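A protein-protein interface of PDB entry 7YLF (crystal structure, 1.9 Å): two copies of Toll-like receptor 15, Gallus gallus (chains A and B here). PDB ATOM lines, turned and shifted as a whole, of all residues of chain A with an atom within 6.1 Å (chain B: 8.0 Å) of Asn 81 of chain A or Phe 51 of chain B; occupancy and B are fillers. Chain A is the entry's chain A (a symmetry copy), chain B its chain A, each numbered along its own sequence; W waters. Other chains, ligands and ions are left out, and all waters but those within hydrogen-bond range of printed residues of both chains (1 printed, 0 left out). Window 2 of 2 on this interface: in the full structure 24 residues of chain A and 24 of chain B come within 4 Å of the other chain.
The backbone NH (N) of Ile 61 of chain B lies within hydrogen-bond range of the side-chain amide oxygen (OE1) of Gln 86 of chain A (3.0 Å).
The backbone carbonyl oxygen (O) of Gly 59 of chain B sits at hydrogen-bond distance from the side-chain amide nitrogen (NE2) of Gln 86 of chain A (2.9 Å).
SG of Cys 45 of chain B forms a disulfide with SG of Cys 64 of chain B (2.0 Å).
The side-chain amide nitrogen (ND2) of Asn 81 of chain A is in hydrogen-bond range of the backbone carbonyl oxygen (O) of Pro 77 of chain A (3.2 Å).
The side-chain amide oxygen (OD1) of Asn 60 of chain B sits at hydrogen-bond distance from the backbone NH (N) of Phe 62 of chain B.
The backbone carbonyl oxygen of Lys 52 of chain B sits close to the backbone NH of Gly 59 of chain B.
OD1 of Asn 60 of chain B sits at hydrogen-bond distance from N of Tyr 63 of chain B (3.5 Å).
O of Val 80 of chain A sits at hydrogen-bond distance from NE2 of Gln 86 of chain A, at 2.8 Å.
Among the printed residues, pairs that only touch across the chains: Gln 86 of chain A with Asn 60 of chain B, Asn 81 of chain A with Phe 51 of chain B, Cys 83 of chain A with His 47 of chain B, Cys 83 of chain A with Phe 51 of chain B, Cys 83 of chain A with Ile 61 of chain B, Asn 81 of chain A with Gly 54 of chain B, Asn 81 of chain A with Pro 53 of chain B and Gln 86 of chain A with Phe 51 of chain B.
Printed residues of chain B within 4 Å of Asn 81 of chain A: Phe 51, Pro 53 and Gly 54.
Of the printed residues of chain A, Phe 51 of chain B touches Asn 81, Cys 83 and Gln 86.
Printed residues of chain A within 4 Å of Gly 54 of chain B: Asn 81 (3.8 Å).
Of the printed residues of chain B, Cys 83 of chain A touches His 47 (3.6 Å), Phe 51 (3.6 Å) and Ile 61 (3.6 Å).
Of the printed residues of chain A, His 47 of chain B touches Cys 83.
The nearest residue of chain B that does not touch Asn 81 of chain A is Gly 59 of chain B (4.8 Å).
The nearest printed residue of chain A that does not touch Phe 51 of chain B is Ser 82 of chain A (4.2 Å).
The nearest printed residue of chain A that does not touch Gly 54 of chain B is Ser 82 of chain A (6.5 Å).
Of the 20 printed residues of chain B, 7 touch a printed residue of chain A.
Among the printed residues, no Asp or Glu carboxylate lies within 4 Å of a Lys or Arg side-chain nitrogen of the other chain.
No position is printed for both chains.
Of the 10 pairs that touch across the chains among the printed residues, none has its exchanged pair printed and touching as well.
Water W1 lies within hydrogen-bond range of the backbone carbonyl oxygen (O) of Gly 59 of chain B (2.6 Å), the backbone NH (N) of Gly 54 of chain B (2.8 Å) and the backbone carbonyl oxygen (O) of Asn 81 of chain A (3.2 Å).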
ATOM      1  N   SER A  76     -22.977  21.922  17.343  1.00  0.00           N
ATOM      2  CA  SER A  76     -21.555  21.659  17.514  1.00  0.00           C
ATOM      3  C   SER A  76     -21.433  20.381  18.326  1.00  0.00           C
ATOM      4  O   SER A  76     -22.430  19.894  18.863  1.00  0.00           O
ATOM      5  CB  SER A  76     -20.855  22.819  18.235  1.00  0.00           C
ATOM      6  OG  SER A  76     -21.335  22.903  19.564  1.00  0.00           O
ATOM      7  N   PRO A  77     -20.230  19.802  18.433  1.00  0.00           N
ATOM      8  CA  PRO A  77     -20.077  18.680  19.381  1.00  0.00           C
ATOM      9  C   PRO A  77     -20.585  19.000  20.776  1.00  0.00           C
ATOM     10  O   PRO A  77     -21.237  18.153  21.395  1.00  0.00           O
ATOM     11  CB  PRO A  77     -18.569  18.419  19.360  1.00  0.00           C
ATOM     12  CG  PRO A  77     -18.173  18.772  17.946  1.00  0.00           C
ATOM     13  CD  PRO A  77     -19.024  19.980  17.604  1.00  0.00           C
ATOM     14  N   SER A  78     -20.340  20.217  21.276  1.00  0.00           N
ATOM     15  CA  SER A  78     -20.779  20.553  22.627  1.00  0.00           C
ATOM     16  C   SER A  78     -22.290  20.489  22.754  1.00  0.00           C
ATOM     17  O   SER A  78     -22.805  20.118  23.814  1.00  0.00           O
ATOM     18  CB  SER A  78     -20.264  21.938  23.021  1.00  0.00           C
ATOM     19  OG  SER A  78     -20.943  22.950  22.291  1.00  0.00           O
ATOM     20  N   PHE A  79     -23.019  20.838  21.684  1.00  0.00           N
ATOM     21  CA  PHE A  79     -24.473  20.714  21.695  1.00  0.00           C
ATOM     22  C   PHE A  79     -24.904  19.249  21.712  1.00  0.00           C
ATOM     23  O   PHE A  79     -25.707  18.835  22.558  1.00  0.00           O
ATOM     24  CB  PHE A  79     -25.046  21.434  20.469  1.00  0.00           C
ATOM     25  CG  PHE A  79     -26.551  21.441  20.411  1.00  0.00           C
ATOM     26  CD1 PHE A  79     -27.245  20.345  19.913  1.00  0.00           C
ATOM     27  CD2 PHE A  79     -27.268  22.544  20.846  1.00  0.00           C
ATOM     28  CE1 PHE A  79     -28.622  20.346  19.864  1.00  0.00           C
ATOM     29  CE2 PHE A  79     -28.651  22.558  20.789  1.00  0.00           C
ATOM     30  CZ  PHE A  79     -29.323  21.462  20.287  1.00  0.00           C
ATOM     31  N   VAL A  80     -24.384  18.451  20.773  1.00  0.00           N
ATOM     32  CA  VAL A  80     -24.822  17.060  20.646  1.00  0.00           C
ATOM     33  C   VAL A  80     -24.488  16.258  21.905  1.00  0.00           C
ATOM     34  O   VAL A  80     -25.258  15.380  22.316  1.00  0.00           O
ATOM     35  CB  VAL A  80     -24.199  16.429  19.381  1.00  0.00           C
ATOM     36  CG1 VAL A  80     -24.430  14.915  19.350  1.00  0.00           C
ATOM     37  CG2 VAL A  80     -24.783  17.079  18.119  1.00  0.00           C
ATOM     38  N   ASN A  81     -23.363  16.551  22.550  1.00  0.00           N
ATOM     39  CA  ASN A  81     -22.947  15.786  23.730  1.00  0.00           C
ATOM     40  C   ASN A  81     -23.494  16.327  25.041  1.00  0.00           C
ATOM     41  O   ASN A  81     -23.231  15.730  26.098  1.00  0.00           O
ATOM     42  CB  ASN A  81     -21.431  15.735  23.826  1.00  0.00           C
ATOM     43  CG  ASN A  81     -20.809  15.090  22.627  1.00  0.00           C
ATOM     44  OD1 ASN A  81     -21.407  14.222  22.002  1.00  0.00           O
ATOM     45  ND2 ASN A  81     -19.605  15.510  22.291  1.00  0.00           N
ATOM     46  N   SER A  82     -24.221  17.433  25.013  1.00  0.00           N
ATOM     47  CA  SER A  82     -24.771  18.005  26.233  1.00  0.00           C
ATOM     48  C   SER A  82     -26.078  17.313  26.601  1.00  0.00           C
ATOM     49  O   SER A  82     -26.986  17.201  25.776  1.00  0.00           O
ATOM     50  CB  SER A  82     -25.013  19.504  26.059  1.00  0.00           C
ATOM     51  OG  SER A  82     -25.872  19.997  27.076  1.00  0.00           O
ATOM     52  N   CYS A  83     -26.160  16.851  27.847  1.00  0.00           N
ATOM     53  CA  CYS A  83     -27.393  16.282  28.376  1.00  0.00           C
ATOM     54  C   CYS A  83     -28.565  17.246  28.194  1.00  0.00           C
ATOM     55  O   CYS A  83     -29.634  16.874  27.693  1.00  0.00           O
ATOM     56  CB  CYS A  83     -27.175  15.951  29.854  1.00  0.00           C
ATOM     57  SG  CYS A  83     -28.610  15.440  30.728  1.00  0.00           S
ATOM     58  N   TRP A  84     -28.365  18.498  28.560  1.00  0.00           N
ATOM     59  CA  TRP A  84     -29.441  19.484  28.466  1.00  0.00           C
ATOM     60  C   TRP A  84     -29.861  19.751  27.034  1.00  0.00           C
ATOM     61  O   TRP A  84     -31.052  19.877  26.742  1.00  0.00           O
ATOM     62  CB  TRP A  84     -29.026  20.786  29.153  1.00  0.00           C
ATOM     63  CG  TRP A  84     -28.731  20.555  30.593  1.00  0.00           C
ATOM     64  CD1 TRP A  84     -27.606  20.923  31.270  1.00  0.00           C
ATOM     65  CD2 TRP A  84     -29.554  19.846  31.531  1.00  0.00           C
ATOM     66  NE1 TRP A  84     -27.691  20.517  32.579  1.00  0.00           N
ATOM     67  CE2 TRP A  84     -28.875  19.849  32.763  1.00  0.00           C
ATOM     68  CE3 TRP A  84     -30.809  19.231  31.453  1.00  0.00           C
ATOM     69  CZ2 TRP A  84     -29.403  19.253  33.906  1.00  0.00           C
ATOM     70  CZ3 TRP A  84     -31.329  18.634  32.588  1.00  0.00           C
ATOM     71  CH2 TRP A  84     -30.629  18.651  33.796  1.00  0.00           C
ATOM     72  N   GLN A  86     -29.662  17.641  24.589  1.00  0.00           N
ATOM     73  CA  GLN A  86     -30.381  16.493  24.079  1.00  0.00           C
ATOM     74  C   GLN A  86     -31.856  16.572  24.522  1.00  0.00           C
ATOM     75  O   GLN A  86     -32.748  16.205  23.773  1.00  0.00           O
ATOM     76  CB  GLN A  86     -29.724  15.178  24.560  1.00  0.00           C
ATOM     77  CG  GLN A  86     -28.390  14.922  23.825  1.00  0.00           C
ATOM     78  CD  GLN A  86     -27.770  13.591  24.239  1.00  0.00           C
ATOM     79  OE1 GLN A  86     -28.461  12.725  24.751  1.00  0.00           O
ATOM     80  NE2 GLN A  86     -26.469  13.430  24.002  1.00  0.00           N
ATOM     81  N   SER A 116     -22.410  10.727  15.684  1.00  0.00           N
ATOM     82  CA  SER A 116     -22.315  11.218  17.053  1.00  0.00           C
ATOM     83  C   SER A 116     -23.680  11.562  17.633  1.00  0.00           C
ATOM     84  O   SER A 116     -23.851  11.533  18.858  1.00  0.00           O
ATOM     85  CB  SER A 116     -21.396  12.441  17.108  1.00  0.00           C
ATOM     86  OG  SER A 116     -21.764  13.398  16.121  1.00  0.00           O
ATOM     87  N   CYS B  45     -29.691   5.164  38.559  1.00  0.00           N
ATOM     88  CA  CYS B  45     -29.065   5.855  37.438  1.00  0.00           C
ATOM     89  C   CYS B  45     -29.446   7.323  37.545  1.00  0.00           C
ATOM     90  O   CYS B  45     -30.632   7.647  37.655  1.00  0.00           O
ATOM     91  CB  CYS B  45     -29.544   5.275  36.094  1.00  0.00           C
ATOM     92  SG  CYS B  45     -28.466   5.567  34.625  1.00  0.00           S
ATOM     93  N   TYR B  46     -28.452   8.208  37.561  1.00  0.00           N
ATOM     94  CA  TYR B  46     -28.763   9.630  37.546  1.00  0.00           C
ATOM     95  C   TYR B  46     -27.652  10.367  36.810  1.00  0.00           C
ATOM     96  O   TYR B  46     -26.484   9.980  36.890  1.00  0.00           O
ATOM     97  CB  TYR B  46     -28.986  10.193  38.963  1.00  0.00           C
ATOM     98  CG  TYR B  46     -27.824  10.161  39.923  1.00  0.00           C
ATOM     99  CD1 TYR B  46     -27.520   9.001  40.648  1.00  0.00           C
ATOM    100  CD2 TYR B  46     -27.057  11.298  40.155  1.00  0.00           C
ATOM    101  CE1 TYR B  46     -26.471   8.975  41.555  1.00  0.00           C
ATOM    102  CE2 TYR B  46     -26.005  11.277  41.060  1.00  0.00           C
ATOM    103  CZ  TYR B  46     -25.715  10.114  41.751  1.00  0.00           C
ATOM    104  OH  TYR B  46     -24.675  10.099  42.646  1.00  0.00           O
ATOM    105  N   HIS B  47     -28.037  11.421  36.083  1.00  0.00           N
ATOM    106  CA  HIS B  47     -27.163  11.989  35.056  1.00  0.00           C
ATOM    107  C   HIS B  47     -25.934  12.650  35.657  1.00  0.00           C
ATOM    108  O   HIS B  47     -24.851  12.612  35.058  1.00  0.00           O
ATOM    109  CB  HIS B  47     -27.930  13.004  34.197  1.00  0.00           C
ATOM    110  CG  HIS B  47     -28.915  12.380  33.256  1.00  0.00           C
ATOM    111  ND1 HIS B  47     -28.772  11.100  32.758  1.00  0.00           N
ATOM    112  CD2 HIS B  47     -30.065  12.859  32.731  1.00  0.00           C
ATOM    113  CE1 HIS B  47     -29.787  10.827  31.956  1.00  0.00           C
ATOM    114  NE2 HIS B  47     -30.596  11.872  31.940  1.00  0.00           N
ATOM    115  N   GLU B  48     -26.075  13.276  36.829  1.00  0.00           N
ATOM    116  CA  GLU B  48     -24.934  13.961  37.427  1.00  0.00           C
ATOM    117  C   GLU B  48     -23.742  13.022  37.577  1.00  0.00           C
ATOM    118  O   GLU B  48     -22.592  13.438  37.402  1.00  0.00           O
ATOM    119  CB  GLU B  48     -25.329  14.568  38.772  1.00  0.00           C
ATOM    120  CG  GLU B  48     -24.316  15.575  39.290  1.00  0.00           C
ATOM    121  CD  GLU B  48     -24.700  16.184  40.628  1.00  0.00           C
ATOM    122  OE1 GLU B  48     -25.873  16.053  41.059  1.00  0.00           O
ATOM    123  OE2 GLU B  48     -23.811  16.799  41.251  1.00  0.00           O
ATOM    124  N   ARG B  49     -23.995  11.748  37.879  1.00  0.00           N
ATOM    125  CA  ARG B  49     -22.933  10.754  37.973  1.00  0.00           C
ATOM    126  C   ARG B  49     -22.793   9.897  36.723  1.00  0.00           C
ATOM    127  O   ARG B  49     -21.670   9.554  36.339  1.00  0.00           O
ATOM    128  CB  ARG B  49     -23.174   9.825  39.173  1.00  0.00           C
ATOM    129  CG  ARG B  49     -22.024   8.852  39.440  1.00  0.00           C
ATOM    130  CD  ARG B  49     -22.400   7.841  40.520  1.00  0.00           C
ATOM    131  NE  ARG B  49     -23.601   7.125  40.121  1.00  0.00           N
ATOM    132  CZ  ARG B  49     -24.386   6.444  40.948  1.00  0.00           C
ATOM    133  NH1 ARG B  49     -24.103   6.371  42.244  1.00  0.00           N
ATOM    134  NH2 ARG B  49     -25.469   5.844  40.477  1.00  0.00           N
ATOM    135  N   ASP B  50     -23.902   9.526  36.089  1.00  0.00           N
ATOM    136  CA  ASP B  50     -23.900   8.434  35.128  1.00  0.00           C
ATOM    137  C   ASP B  50     -24.007   8.874  33.676  1.00  0.00           C
ATOM    138  O   ASP B  50     -23.975   8.014  32.791  1.00  0.00           O
ATOM    139  CB  ASP B  50     -25.035   7.464  35.441  1.00  0.00           C
ATOM    140  CG  ASP B  50     -24.920   6.883  36.829  1.00  0.00           C
ATOM    141  OD1 ASP B  50     -23.833   6.360  37.170  1.00  0.00           O
ATOM    142  OD2 ASP B  50     -25.902   6.976  37.581  1.00  0.00           O
ATOM    143  N   PHE B  51     -24.147  10.169  33.402  1.00  0.00           N
ATOM    144  CA  PHE B  51     -24.100  10.676  32.033  1.00  0.00           C
ATOM    145  C   PHE B  51     -22.648  10.996  31.712  1.00  0.00           C
ATOM    146  O   PHE B  51     -22.007  11.765  32.434  1.00  0.00           O
ATOM    147  CB  PHE B  51     -24.991  11.910  31.876  1.00  0.00           C
ATOM    148  CG  PHE B  51     -25.118  12.407  30.455  1.00  0.00           C
ATOM    149  CD1 PHE B  51     -24.136  13.221  29.894  1.00  0.00           C
ATOM    150  CD2 PHE B  51     -26.227  12.080  29.689  1.00  0.00           C
ATOM    151  CE1 PHE B  51     -24.265  13.700  28.583  1.00  0.00           C
ATOM    152  CE2 PHE B  51     -26.363  12.551  28.390  1.00  0.00           C
ATOM    153  CZ  PHE B  51     -25.382  13.354  27.837  1.00  0.00           C
ATOM    154  N   LYS B  52     -22.120  10.377  30.661  1.00  0.00           N
ATOM    155  CA  LYS B  52     -20.721  10.547  30.266  1.00  0.00           C
ATOM    156  C   LYS B  52     -20.671  11.229  28.910  1.00  0.00           C
ATOM    157  O   LYS B  52     -20.816  10.552  27.879  1.00  0.00           O
ATOM    158  CB  LYS B  52     -20.016   9.191  30.200  1.00  0.00           C
ATOM    159  CG  LYS B  52     -20.210   8.335  31.461  1.00  0.00           C
ATOM    160  CD  LYS B  52     -19.564   9.001  32.654  1.00  0.00           C
ATOM    161  CE  LYS B  52     -19.543   8.077  33.871  1.00  0.00           C
ATOM    162  NZ  LYS B  52     -18.691   8.660  34.937  1.00  0.00           N
ATOM    163  N   PRO B  53     -20.457  12.545  28.853  1.00  0.00           N
ATOM    164  CA  PRO B  53     -20.489  13.251  27.564  1.00  0.00           C
ATOM    165  C   PRO B  53     -19.584  12.609  26.526  1.00  0.00           C
ATOM    166  O   PRO B  53     -18.418  12.296  26.793  1.00  0.00           O
ATOM    167  CB  PRO B  53     -20.014  14.659  27.929  1.00  0.00           C
ATOM    168  CG  PRO B  53     -20.503  14.841  29.317  1.00  0.00           C
ATOM    169  CD  PRO B  53     -20.367  13.484  29.984  1.00  0.00           C
ATOM    170  N   GLY B  54     -20.130  12.424  25.320  1.00  0.00           N
ATOM    171  CA  GLY B  54     -19.385  11.840  24.224  1.00  0.00           C
ATOM    172  C   GLY B  54     -19.362  10.329  24.217  1.00  0.00           C
ATOM    173  O   GLY B  54     -18.980   9.729  23.205  1.00  0.00           O
ATOM    174  N   HIS B  55     -19.739   9.694  25.314  1.00  0.00           N
ATOM    175  CA  HIS B  55     -19.738   8.241  25.352  1.00  0.00           C
ATOM    176  C   HIS B  55     -20.909   7.721  24.524  1.00  0.00           C
ATOM    177  O   HIS B  55     -22.044   8.181  24.708  1.00  0.00           O
ATOM    178  CB  HIS B  55     -19.839   7.744  26.799  1.00  0.00           C
ATOM    179  CG  HIS B  55     -19.531   6.292  26.957  1.00  0.00           C
ATOM    180  ND1 HIS B  55     -20.366   5.299  26.491  1.00  0.00           N
ATOM    181  CD2 HIS B  55     -18.488   5.661  27.553  1.00  0.00           C
ATOM    182  CE1 HIS B  55     -19.852   4.119  26.797  1.00  0.00           C
ATOM    183  NE2 HIS B  55     -18.702   4.311  27.422  1.00  0.00           N
ATOM    184  N   PRO B  56     -20.680   6.791  23.594  1.00  0.00           N
ATOM    185  CA  PRO B  56     -21.774   6.381  22.692  1.00  0.00           C
ATOM    186  C   PRO B  56     -22.940   5.725  23.405  1.00  0.00           C
ATOM    187  O   PRO B  56     -24.076   5.803  22.920  1.00  0.00           O
ATOM    188  CB  PRO B  56     -21.088   5.419  21.716  1.00  0.00           C
ATOM    189  CG  PRO B  56     -19.783   4.989  22.429  1.00  0.00           C
ATOM    190  CD  PRO B  56     -19.385   6.191  23.231  1.00  0.00           C
ATOM    191  N   VAL B  57     -22.707   5.079  24.541  1.00  0.00           N
ATOM    192  CA  VAL B  57     -23.781   4.472  25.314  1.00  0.00           C
ATOM    193  C   VAL B  57     -24.207   5.358  26.471  1.00  0.00           C
ATOM    194  O   VAL B  57     -25.396   5.583  26.680  1.00  0.00           O
ATOM    195  CB  VAL B  57     -23.346   3.077  25.815  1.00  0.00           C
ATOM    196  CG1 VAL B  57     -24.483   2.403  26.591  1.00  0.00           C
ATOM    197  CG2 VAL B  57     -22.879   2.238  24.643  1.00  0.00           C
ATOM    198  N   LEU B  58     -23.247   5.853  27.251  1.00  0.00           N
ATOM    199  CA  LEU B  58     -23.573   6.569  28.479  1.00  0.00           C
ATOM    200  C   LEU B  58     -23.789   8.062  28.263  1.00  0.00           C
ATOM    201  O   LEU B  58     -24.242   8.744  29.189  1.00  0.00           O
ATOM    202  CB  LEU B  58     -22.464   6.366  29.514  1.00  0.00           C
ATOM    203  CG  LEU B  58     -22.177   4.908  29.866  1.00  0.00           C
ATOM    204  CD1 LEU B  58     -20.991   4.807  30.803  1.00  0.00           C
ATOM    205  CD2 LEU B  58     -23.437   4.293  30.493  1.00  0.00           C
ATOM    206  N   GLY B  59     -23.491   8.574  27.075  1.00  0.00           N
ATOM    207  CA  GLY B  59     -23.635   9.991  26.813  1.00  0.00           C
ATOM    208  C   GLY B  59     -24.899  10.343  26.068  1.00  0.00           C
ATOM    209  O   GLY B  59     -24.900  11.262  25.241  1.00  0.00           O
ATOM    210  N   ASN B  60     -25.992   9.635  26.325  1.00  0.00           N
ATOM    211  CA  ASN B  60     -27.254  10.157  25.826  1.00  0.00           C
ATOM    212  C   ASN B  60     -28.349   9.927  26.850  1.00  0.00           C
ATOM    213  O   ASN B  60     -28.255   9.056  27.719  1.00  0.00           O
ATOM    214  CB  ASN B  60     -27.636   9.575  24.462  1.00  0.00           C
ATOM    215  CG  ASN B  60     -28.063   8.140  24.535  1.00  0.00           C
ATOM    216  OD1 ASN B  60     -29.177   7.837  24.954  1.00  0.00           O
ATOM    217  ND2 ASN B  60     -27.201   7.248  24.085  1.00  0.00           N
ATOM    218  N   ILE B  61     -29.396  10.745  26.731  1.00  0.00           N
ATOM    219  CA  ILE B  61     -30.427  10.823  27.758  1.00  0.00           C
ATOM    220  C   ILE B  61     -31.334   9.607  27.788  1.00  0.00           C
ATOM    221  O   ILE B  61     -32.123   9.468  28.730  1.00  0.00           O
ATOM    222  CB  ILE B  61     -31.293  12.084  27.559  1.00  0.00           C
ATOM    223  CG1 ILE B  61     -31.857  12.134  26.138  1.00  0.00           C
ATOM    224  CG2 ILE B  61     -30.466  13.359  27.796  1.00  0.00           C
ATOM    225  CD1 ILE B  61     -32.987  13.150  26.008  1.00  0.00           C
ATOM    226  N   PHE B  62     -31.277   8.747  26.773  1.00  0.00           N
ATOM    227  CA  PHE B  62     -32.132   7.566  26.779  1.00  0.00           C
ATOM    228  C   PHE B  62     -31.573   6.448  27.643  1.00  0.00           C
ATOM    229  O   PHE B  62     -32.325   5.534  28.015  1.00  0.00           O
ATOM    230  CB  PHE B  62     -32.328   7.055  25.353  1.00  0.00           C
ATOM    231  CG  PHE B  62     -33.038   8.043  24.460  1.00  0.00           C
ATOM    232  CD1 PHE B  62     -34.417   8.122  24.461  1.00  0.00           C
ATOM    233  CD2 PHE B  62     -32.321   8.894  23.647  1.00  0.00           C
ATOM    234  CE1 PHE B  62     -35.074   9.035  23.642  1.00  0.00           C
ATOM    235  CE2 PHE B  62     -32.968   9.800  22.837  1.00  0.00           C
ATOM    236  CZ  PHE B  62     -34.354   9.864  22.847  1.00  0.00           C
ATOM    237  N   TYR B  63     -30.284   6.498  27.979  1.00  0.00           N
ATOM    238  CA  TYR B  63     -29.662   5.352  28.642  1.00  0.00           C
ATOM    239  C   TYR B  63     -30.311   5.054  29.995  1.00  0.00           C
ATOM    240  O   TYR B  63     -30.721   3.916  30.261  1.00  0.00           O
ATOM    241  CB  TYR B  63     -28.163   5.576  28.814  1.00  0.00           C
ATOM    242  CG  TYR B  63     -27.519   4.509  29.705  1.00  0.00           C
ATOM    243  CD1 TYR B  63     -27.199   3.256  29.202  1.00  0.00           C
ATOM    244  CD2 TYR B  63     -27.265   4.762  31.051  1.00  0.00           C
ATOM    245  CE1 TYR B  63     -26.602   2.252  30.034  1.00  0.00           C
ATOM    246  CE2 TYR B  63     -26.687   3.785  31.876  1.00  0.00           C
ATOM    247  CZ  TYR B  63     -26.357   2.542  31.360  1.00  0.00           C
ATOM    248  OH  TYR B  63     -25.786   1.599  32.196  1.00  0.00           O
ATOM    249  N   CYS B  64     -30.370   6.046  30.891  1.00  0.00           N
ATOM    250  CA  CYS B  64     -30.869   5.752  32.238  1.00  0.00           C
ATOM    251  C   CYS B  64     -32.313   5.285  32.191  1.00  0.00           C
ATOM    252  O   CYS B  64     -32.667   4.255  32.776  1.00  0.00           O
ATOM    253  CB  CYS B  64     -30.755   6.971  33.157  1.00  0.00           C
ATOM    254  SG  CYS B  64     -29.124   7.341  33.851  1.00  0.00           S
HETATM  255  O   HOH W   1     -22.846  12.763  24.909  1.00  0.00           O
